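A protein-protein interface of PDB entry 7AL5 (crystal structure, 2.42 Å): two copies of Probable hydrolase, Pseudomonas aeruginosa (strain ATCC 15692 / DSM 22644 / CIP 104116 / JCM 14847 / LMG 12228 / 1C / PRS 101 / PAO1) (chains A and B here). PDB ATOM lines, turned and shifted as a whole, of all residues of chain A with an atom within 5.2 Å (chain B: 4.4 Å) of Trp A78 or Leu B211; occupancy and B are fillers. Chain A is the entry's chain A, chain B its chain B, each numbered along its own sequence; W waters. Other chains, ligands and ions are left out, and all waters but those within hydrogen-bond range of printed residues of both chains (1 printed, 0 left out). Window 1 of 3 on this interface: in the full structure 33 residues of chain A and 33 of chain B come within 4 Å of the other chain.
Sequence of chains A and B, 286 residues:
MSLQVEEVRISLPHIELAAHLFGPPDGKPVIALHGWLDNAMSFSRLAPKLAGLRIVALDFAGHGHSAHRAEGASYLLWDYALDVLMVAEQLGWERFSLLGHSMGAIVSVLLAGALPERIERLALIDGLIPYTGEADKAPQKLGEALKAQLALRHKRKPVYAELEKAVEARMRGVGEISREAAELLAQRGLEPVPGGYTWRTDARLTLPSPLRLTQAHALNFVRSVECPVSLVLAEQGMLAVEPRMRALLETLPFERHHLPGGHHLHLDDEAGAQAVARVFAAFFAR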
ATOM      1  N   LEU A  76      -6.521  -7.240   6.424  1.00  0.00           N
ATOM      2  CA  LEU A  76      -7.155  -8.347   7.115  1.00  0.00           C
ATOM      3  C   LEU A  76      -6.670  -8.413   8.548  1.00  0.00           C
ATOM      4  O   LEU A  76      -5.645  -7.845   8.902  1.00  0.00           O
ATOM      5  CB  LEU A  76      -6.873  -9.664   6.405  1.00  0.00           C
ATOM      6  CG  LEU A  76      -7.291  -9.568   4.931  1.00  0.00           C
ATOM      7  CD1 LEU A  76      -7.014 -10.861   4.193  1.00  0.00           C
ATOM      8  CD2 LEU A  76      -8.753  -9.153   4.800  1.00  0.00           C
ATOM      9  N   LEU A  77      -7.448  -9.104   9.395  1.00  0.00           N
ATOM     10  CA  LEU A  77      -7.147  -9.067  10.824  1.00  0.00           C
ATOM     11  C   LEU A  77      -5.748  -9.570  11.098  1.00  0.00           C
ATOM     12  O   LEU A  77      -5.098  -9.089  12.030  1.00  0.00           O
ATOM     13  CB  LEU A  77      -8.159  -9.881  11.632  1.00  0.00           C
ATOM     14  CG  LEU A  77      -9.532  -9.219  11.643  1.00  0.00           C
ATOM     15  CD1 LEU A  77     -10.603 -10.140  12.219  1.00  0.00           C
ATOM     16  CD2 LEU A  77      -9.512  -7.901  12.387  1.00  0.00           C
ATOM     17  N   TRP A  78      -5.300 -10.595  10.379  1.00  0.00           N
ATOM     18  CA  TRP A  78      -3.955 -11.195  10.567  1.00  0.00           C
ATOM     19  C   TRP A  78      -2.851 -10.288  10.016  1.00  0.00           C
ATOM     20  O   TRP A  78      -1.736 -10.452  10.425  1.00  0.00           O
ATOM     21  CB  TRP A  78      -3.869 -12.638  10.075  1.00  0.00           C
ATOM     22  CG  TRP A  78      -4.383 -12.827   8.697  1.00  0.00           C
ATOM     23  CD1 TRP A  78      -3.695 -12.681   7.543  1.00  0.00           C
ATOM     24  CD2 TRP A  78      -5.721 -13.168   8.336  1.00  0.00           C
ATOM     25  NE1 TRP A  78      -4.513 -12.923   6.489  1.00  0.00           N
ATOM     26  CE2 TRP A  78      -5.756 -13.227   6.943  1.00  0.00           C
ATOM     27  CE3 TRP A  78      -6.886 -13.420   9.052  1.00  0.00           C
ATOM     28  CZ2 TRP A  78      -6.913 -13.537   6.247  1.00  0.00           C
ATOM     29  CZ3 TRP A  78      -8.031 -13.724   8.365  1.00  0.00           C
ATOM     30  CH2 TRP A  78      -8.043 -13.775   6.981  1.00  0.00           C
ATOM     31  N   ASP A  79      -3.126  -9.415   9.058  1.00  0.00           N
ATOM     32  CA  ASP A  79      -2.109  -8.436   8.686  1.00  0.00           C
ATOM     33  C   ASP A  79      -1.780  -7.534   9.869  1.00  0.00           C
ATOM     34  O   ASP A  79      -0.614  -7.219  10.098  1.00  0.00           O
ATOM     35  CB  ASP A  79      -2.551  -7.617   7.475  1.00  0.00           C
ATOM     36  CG  ASP A  79      -2.882  -8.487   6.258  1.00  0.00           C
ATOM     37  OD1 ASP A  79      -2.116  -9.455   5.952  1.00  0.00           O
ATOM     38  OD2 ASP A  79      -3.938  -8.177   5.634  1.00  0.00           O
ATOM     39  N   TYR A  80      -2.768  -7.158  10.679  1.00  0.00           N
ATOM     40  CA  TYR A  80      -2.557  -6.340  11.899  1.00  0.00           C
ATOM     41  C   TYR A  80      -1.734  -7.132  12.917  1.00  0.00           C
ATOM     42  O   TYR A  80      -0.869  -6.575  13.525  1.00  0.00           O
ATOM     43  CB  TYR A  80      -3.859  -5.896  12.559  1.00  0.00           C
ATOM     44  CG  TYR A  80      -4.684  -4.884  11.814  1.00  0.00           C
ATOM     45  CD1 TYR A  80      -4.153  -3.686  11.376  1.00  0.00           C
ATOM     46  CD2 TYR A  80      -6.023  -5.132  11.583  1.00  0.00           C
ATOM     47  CE1 TYR A  80      -4.931  -2.766  10.710  1.00  0.00           C
ATOM     48  CE2 TYR A  80      -6.814  -4.227  10.920  1.00  0.00           C
ATOM     49  CZ  TYR A  80      -6.269  -3.039  10.491  1.00  0.00           C
ATOM     50  OH  TYR A  80      -7.085  -2.172   9.857  1.00  0.00           O
ATOM     51  N   ALA A  81      -2.031  -8.413  13.077  1.00  0.00           N
ATOM     52  CA  ALA A  81      -1.295  -9.271  13.995  1.00  0.00           C
ATOM     53  C   ALA A  81       0.190  -9.276  13.675  1.00  0.00           C
ATOM     54  O   ALA A  81       1.031  -9.093  14.556  1.00  0.00           O
ATOM     55  CB  ALA A  81      -1.844 -10.690  13.932  1.00  0.00           C
ATOM     56  N   LEU A  82       0.533  -9.465  12.409  1.00  0.00           N
ATOM     57  CA  LEU A  82       1.927  -9.362  12.017  1.00  0.00           C
ATOM     58  C   LEU A  82       2.516  -7.995  12.380  1.00  0.00           C
ATOM     59  O   LEU A  82       3.624  -7.928  12.914  1.00  0.00           O
ATOM     60  CB  LEU A  82       2.070  -9.639  10.517  1.00  0.00           C
ATOM     61  CG  LEU A  82       3.516  -9.572  10.002  1.00  0.00           C
ATOM     62  CD1 LEU A  82       4.454 -10.546  10.761  1.00  0.00           C
ATOM     63  CD2 LEU A  82       3.569  -9.840   8.515  1.00  0.00           C
ATOM     64  N   LEU A 110      -6.252 -13.253  18.266  1.00  0.00           N
ATOM     65  CA  LEU A 110      -5.619 -13.955  17.168  1.00  0.00           C
ATOM     66  C   LEU A 110      -4.141 -14.117  17.452  1.00  0.00           C
ATOM     67  O   LEU A 110      -3.574 -15.212  17.328  1.00  0.00           O
ATOM     68  CB  LEU A 110      -5.838 -13.195  15.863  1.00  0.00           C
ATOM     69  CG  LEU A 110      -7.248 -13.211  15.297  1.00  0.00           C
ATOM     70  CD1 LEU A 110      -7.208 -12.742  13.832  1.00  0.00           C
ATOM     71  CD2 LEU A 110      -7.883 -14.573  15.373  1.00  0.00           C
ATOM     72  N   SER A 209     -14.151  -8.649   3.576  1.00  0.00           N
ATOM     73  CA  SER A 209     -13.107  -9.666   3.569  1.00  0.00           C
ATOM     74  C   SER A 209     -13.280 -10.579   2.361  1.00  0.00           C
ATOM     75  O   SER A 209     -14.406 -10.958   2.011  1.00  0.00           O
ATOM     76  CB  SER A 209     -13.153 -10.498   4.848  1.00  0.00           C
ATOM     77  OG  SER A 209     -12.003 -11.315   4.962  1.00  0.00           O
ATOM     78  N   LEU A 211     -12.217 -13.570   2.516  1.00  0.00           N
ATOM     79  CA  LEU A 211     -12.393 -14.896   3.125  1.00  0.00           C
ATOM     80  C   LEU A 211     -12.545 -14.725   4.632  1.00  0.00           C
ATOM     81  O   LEU A 211     -11.553 -14.509   5.333  1.00  0.00           O
ATOM     82  CB  LEU A 211     -11.228 -15.820   2.801  1.00  0.00           C
ATOM     83  CG  LEU A 211     -11.269 -17.173   3.529  1.00  0.00           C
ATOM     84  CD1 LEU A 211     -12.265 -18.151   2.906  1.00  0.00           C
ATOM     85  CD2 LEU A 211      -9.876 -17.821   3.599  1.00  0.00           C
ATOM     86  N   ARG A 212     -13.776 -14.861   5.122  1.00  0.00           N
ATOM     87  CA  ARG A 212     -14.068 -14.726   6.537  1.00  0.00           C
ATOM     88  C   ARG A 212     -13.648 -15.969   7.305  1.00  0.00           C
ATOM     89  O   ARG A 212     -13.677 -17.090   6.779  1.00  0.00           O
ATOM     90  CB  ARG A 212     -15.563 -14.481   6.755  1.00  0.00           C
ATOM     91  CG  ARG A 212     -15.887 -12.998   6.893  1.00  0.00           C
ATOM     92  CD  ARG A 212     -17.357 -12.717   7.022  1.00  0.00           C
ATOM     93  NE  ARG A 212     -17.605 -11.573   7.896  1.00  0.00           N
ATOM     94  CZ  ARG A 212     -18.564 -10.672   7.685  1.00  0.00           C
ATOM     95  NH1 ARG A 212     -19.362 -10.783   6.624  1.00  0.00           N
ATOM     96  NH2 ARG A 212     -18.732  -9.657   8.531  1.00  0.00           N
ATOM     97  N   LEU A 213     -13.257 -15.758   8.563  1.00  0.00           N
ATOM     98  CA  LEU A 213     -13.047 -16.871   9.472  1.00  0.00           C
ATOM     99  C   LEU A 213     -14.380 -17.560   9.722  1.00  0.00           C
ATOM    100  O   LEU A 213     -15.405 -16.894   9.915  1.00  0.00           O
ATOM    101  CB  LEU A 213     -12.462 -16.396  10.796  1.00  0.00           C
ATOM    102  CG  LEU A 213     -11.054 -15.809  10.774  1.00  0.00           C
ATOM    103  CD1 LEU A 213     -10.771 -15.126  12.101  1.00  0.00           C
ATOM    104  CD2 LEU A 213     -10.016 -16.856  10.518  1.00  0.00           C
ATOM    105  N   HIS A 217     -13.115 -21.508  13.299  1.00  0.00           N
ATOM    106  CA  HIS A 217     -11.878 -20.750  13.385  1.00  0.00           C
ATOM    107  C   HIS A 217     -11.875 -19.854  14.619  1.00  0.00           C
ATOM    108  O   HIS A 217     -10.976 -19.935  15.463  1.00  0.00           O
ATOM    109  CB  HIS A 217     -11.683 -19.932  12.108  1.00  0.00           C
ATOM    110  CG  HIS A 217     -11.205 -20.732  10.942  1.00  0.00           C
ATOM    111  ND1 HIS A 217     -12.040 -21.136   9.923  1.00  0.00           N
ATOM    112  CD2 HIS A 217      -9.980 -21.201  10.627  1.00  0.00           C
ATOM    113  CE1 HIS A 217     -11.348 -21.801   9.022  1.00  0.00           C
ATOM    114  NE2 HIS A 217     -10.093 -21.852   9.425  1.00  0.00           N
ATOM    115  N   TRP B  78      -6.408 -15.568  -3.695  1.00  0.00           N
ATOM    116  CA  TRP B  78      -7.428 -14.601  -4.088  1.00  0.00           C
ATOM    117  C   TRP B  78      -6.854 -13.216  -4.406  1.00  0.00           C
ATOM    118  O   TRP B  78      -7.577 -12.364  -4.928  1.00  0.00           O
ATOM    119  CB  TRP B  78      -8.524 -14.500  -2.991  1.00  0.00           C
ATOM    120  CG  TRP B  78      -8.009 -14.302  -1.609  1.00  0.00           C
ATOM    121  CD1 TRP B  78      -7.703 -13.106  -1.017  1.00  0.00           C
ATOM    122  CD2 TRP B  78      -7.738 -15.317  -0.629  1.00  0.00           C
ATOM    123  NE1 TRP B  78      -7.246 -13.314   0.261  1.00  0.00           N
ATOM    124  CE2 TRP B  78      -7.267 -14.657   0.534  1.00  0.00           C
ATOM    125  CE3 TRP B  78      -7.829 -16.714  -0.622  1.00  0.00           C
ATOM    126  CZ2 TRP B  78      -6.879 -15.343   1.674  1.00  0.00           C
ATOM    127  CZ3 TRP B  78      -7.444 -17.392   0.511  1.00  0.00           C
ATOM    128  CH2 TRP B  78      -6.975 -16.703   1.648  1.00  0.00           C
ATOM    129  N   LEU B 142      -1.420 -20.109  11.621  1.00  0.00           N
ATOM    130  CA  LEU B 142      -1.200 -18.675  11.636  1.00  0.00           C
ATOM    131  C   LEU B 142       0.131 -18.374  12.295  1.00  0.00           C
ATOM    132  O   LEU B 142       0.942 -17.611  11.748  1.00  0.00           O
ATOM    133  CB  LEU B 142      -2.345 -17.938  12.331  1.00  0.00           C
ATOM    134  CG  LEU B 142      -2.095 -16.443  12.448  1.00  0.00           C
ATOM    135  CD1 LEU B 142      -1.812 -15.857  11.069  1.00  0.00           C
ATOM    136  CD2 LEU B 142      -3.275 -15.729  13.141  1.00  0.00           C
ATOM    137  N   SER B 209       0.652 -19.905   3.944  1.00  0.00           N
ATOM    138  CA  SER B 209      -0.577 -19.153   4.081  1.00  0.00           C
ATOM    139  C   SER B 209      -0.898 -18.900   5.549  1.00  0.00           C
ATOM    140  O   SER B 209      -0.665 -19.777   6.392  1.00  0.00           O
ATOM    141  CB  SER B 209      -1.756 -19.900   3.469  1.00  0.00           C
ATOM    142  OG  SER B 209      -2.879 -19.046   3.362  1.00  0.00           O
ATOM    143  N   PRO B 210      -1.502 -17.744   5.872  1.00  0.00           N
ATOM    144  CA  PRO B 210      -1.954 -17.513   7.237  1.00  0.00           C
ATOM    145  C   PRO B 210      -3.258 -18.225   7.528  1.00  0.00           C
ATOM    146  O   PRO B 210      -3.637 -18.349   8.694  1.00  0.00           O
ATOM    147  CB  PRO B 210      -2.199 -15.993   7.264  1.00  0.00           C
ATOM    148  CG  PRO B 210      -1.615 -15.458   5.979  1.00  0.00           C
ATOM    149  CD  PRO B 210      -1.772 -16.568   5.022  1.00  0.00           C
ATOM    150  N   LEU B 211      -4.018 -18.544   6.487  1.00  0.00           N
ATOM    151  CA  LEU B 211      -5.385 -19.028   6.664  1.00  0.00           C
ATOM    152  C   LEU B 211      -5.750 -19.848   5.432  1.00  0.00           C
ATOM    153  O   LEU B 211      -6.092 -19.279   4.392  1.00  0.00           O
ATOM    154  CB  LEU B 211      -6.370 -17.883   6.865  1.00  0.00           C
ATOM    155  CG  LEU B 211      -7.857 -18.296   6.825  1.00  0.00           C
ATOM    156  CD1 LEU B 211      -8.172 -19.091   8.083  1.00  0.00           C
ATOM    157  CD2 LEU B 211      -8.875 -17.172   6.728  1.00  0.00           C
ATOM    158  N   ARG B 212      -5.701 -21.169   5.578  1.00  0.00           N
ATOM    159  CA  ARG B 212      -6.052 -22.083   4.500  1.00  0.00           C
ATOM    160  C   ARG B 212      -7.568 -22.125   4.306  1.00  0.00           C
ATOM    161  O   ARG B 212      -8.340 -21.824   5.216  1.00  0.00           O
ATOM    162  CB  ARG B 212      -5.530 -23.484   4.822  1.00  0.00           C
ATOM    163  CG  ARG B 212      -4.063 -23.708   4.458  1.00  0.00           C
ATOM    164  CD  ARG B 212      -3.623 -25.174   4.610  1.00  0.00           C
ATOM    165  NE  ARG B 212      -2.258 -25.434   4.118  1.00  0.00           N
ATOM    166  CZ  ARG B 212      -1.603 -26.599   4.253  1.00  0.00           C
ATOM    167  NH1 ARG B 212      -2.175 -27.636   4.867  1.00  0.00           N
ATOM    168  NH2 ARG B 212      -0.371 -26.734   3.772  1.00  0.00           N
ATOM    169  N   LEU B 213      -7.988 -22.455   3.084  1.00  0.00           N
ATOM    170  CA  LEU B 213      -9.349 -22.910   2.867  1.00  0.00           C
ATOM    171  C   LEU B 213      -9.568 -24.221   3.601  1.00  0.00           C
ATOM    172  O   LEU B 213      -8.701 -25.098   3.608  1.00  0.00           O
ATOM    173  CB  LEU B 213      -9.630 -23.118   1.377  1.00  0.00           C
ATOM    174  CG  LEU B 213      -9.555 -21.937   0.395  1.00  0.00           C
ATOM    175  CD1 LEU B 213     -10.344 -22.255  -0.875  1.00  0.00           C
ATOM    176  CD2 LEU B 213     -10.100 -20.677   1.025  1.00  0.00           C
HETATM  177  O   HOH W   1      -7.969 -23.118   7.816  1.00  0.00           O
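The side-chain hydroxyl of Ser A209 sits at hydrogen-bond distance from the backbone carbonyl oxygen of Leu A211 (3.2 Å).
OG of Ser B209 sits close to N of Leu B211, 3.4 Å away.
Among the printed residues, merely in contact across the chains: Trp A78 with Leu B142 (3.9 Å), Trp A78 with Pro B210 (3.6 Å), Trp A78 with Leu B211 (3.5 Å), Leu A211 with Trp B78 (3.7 Å), Leu A211 with Leu B211 (3.3 Å), Leu A211 with Leu B213 (3.8 Å), Leu A213 with Leu B211 (3.8 Å) and His A217 with Leu B211 (3.6 Å).
Trp A78 touches just these residues of chain B: Leu B142, Pro B210 and Leu B211.
Tyr A80 touches none of the printed residues of chain B.
Of the printed residues of chain B, Leu A211 touches Trp B78, Leu B211 and Leu B213.
Arg A212 touches none of the printed residues of chain B.
Printed residues of chain B within 4 Å of Leu A213: Leu B211.
Of the printed residues of chain B, His A217 touches Leu B211 (3.6 Å).
Printed residues of chain A within 4 Å of Leu B142: Trp A78.
Leu B211 touches just these residues of chain A: Trp A78 (3.5 Å), Leu A211 (3.3 Å), Leu A213 (3.8 Å) and His A217 (3.6 Å).
Of the printed residues of chain A, Leu B213 touches Leu A211 (3.8 Å).
The nearest printed residue of chain A that does not touch Leu B142 is Leu A110 (4.2 Å).
Hydrophobic or aromatic side chains of chain A within 4 Å of the printed part of chain B: Trp A78, Leu A211, Leu A213 and His A217.
Along chain A the printed residues that touch a printed residue of chain B span positions 78 to 217.
Printed residues of chain B that touch a printed residue of chain A: Trp B78, Leu B142, Pro B210, Leu B211 and Leu B213.
Along chain B the printed residues that touch a printed residue of chain A span positions 78 to 213.
Among the printed residues, no Asp or Glu carboxylate lies within 4 Å of a Lys or Arg side-chain nitrogen of the other chain.
Trp A78 touches Leu B211, and with the chains exchanged Leu A211 touches Trp B78.
Leu B211 touches its own counterpart, Leu A211.
Leu A211 touches Leu B213, and with the chains exchanged Leu A213 touches Leu B211.
Positions printed for both chains: 78, 209, 211, 212 and 213.
Water W1 bridges the backbone carbonyl oxygen (O) of Arg B212 (2.9 Å) and a ring nitrogen (NE2) of His A217 (3.0 Å).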
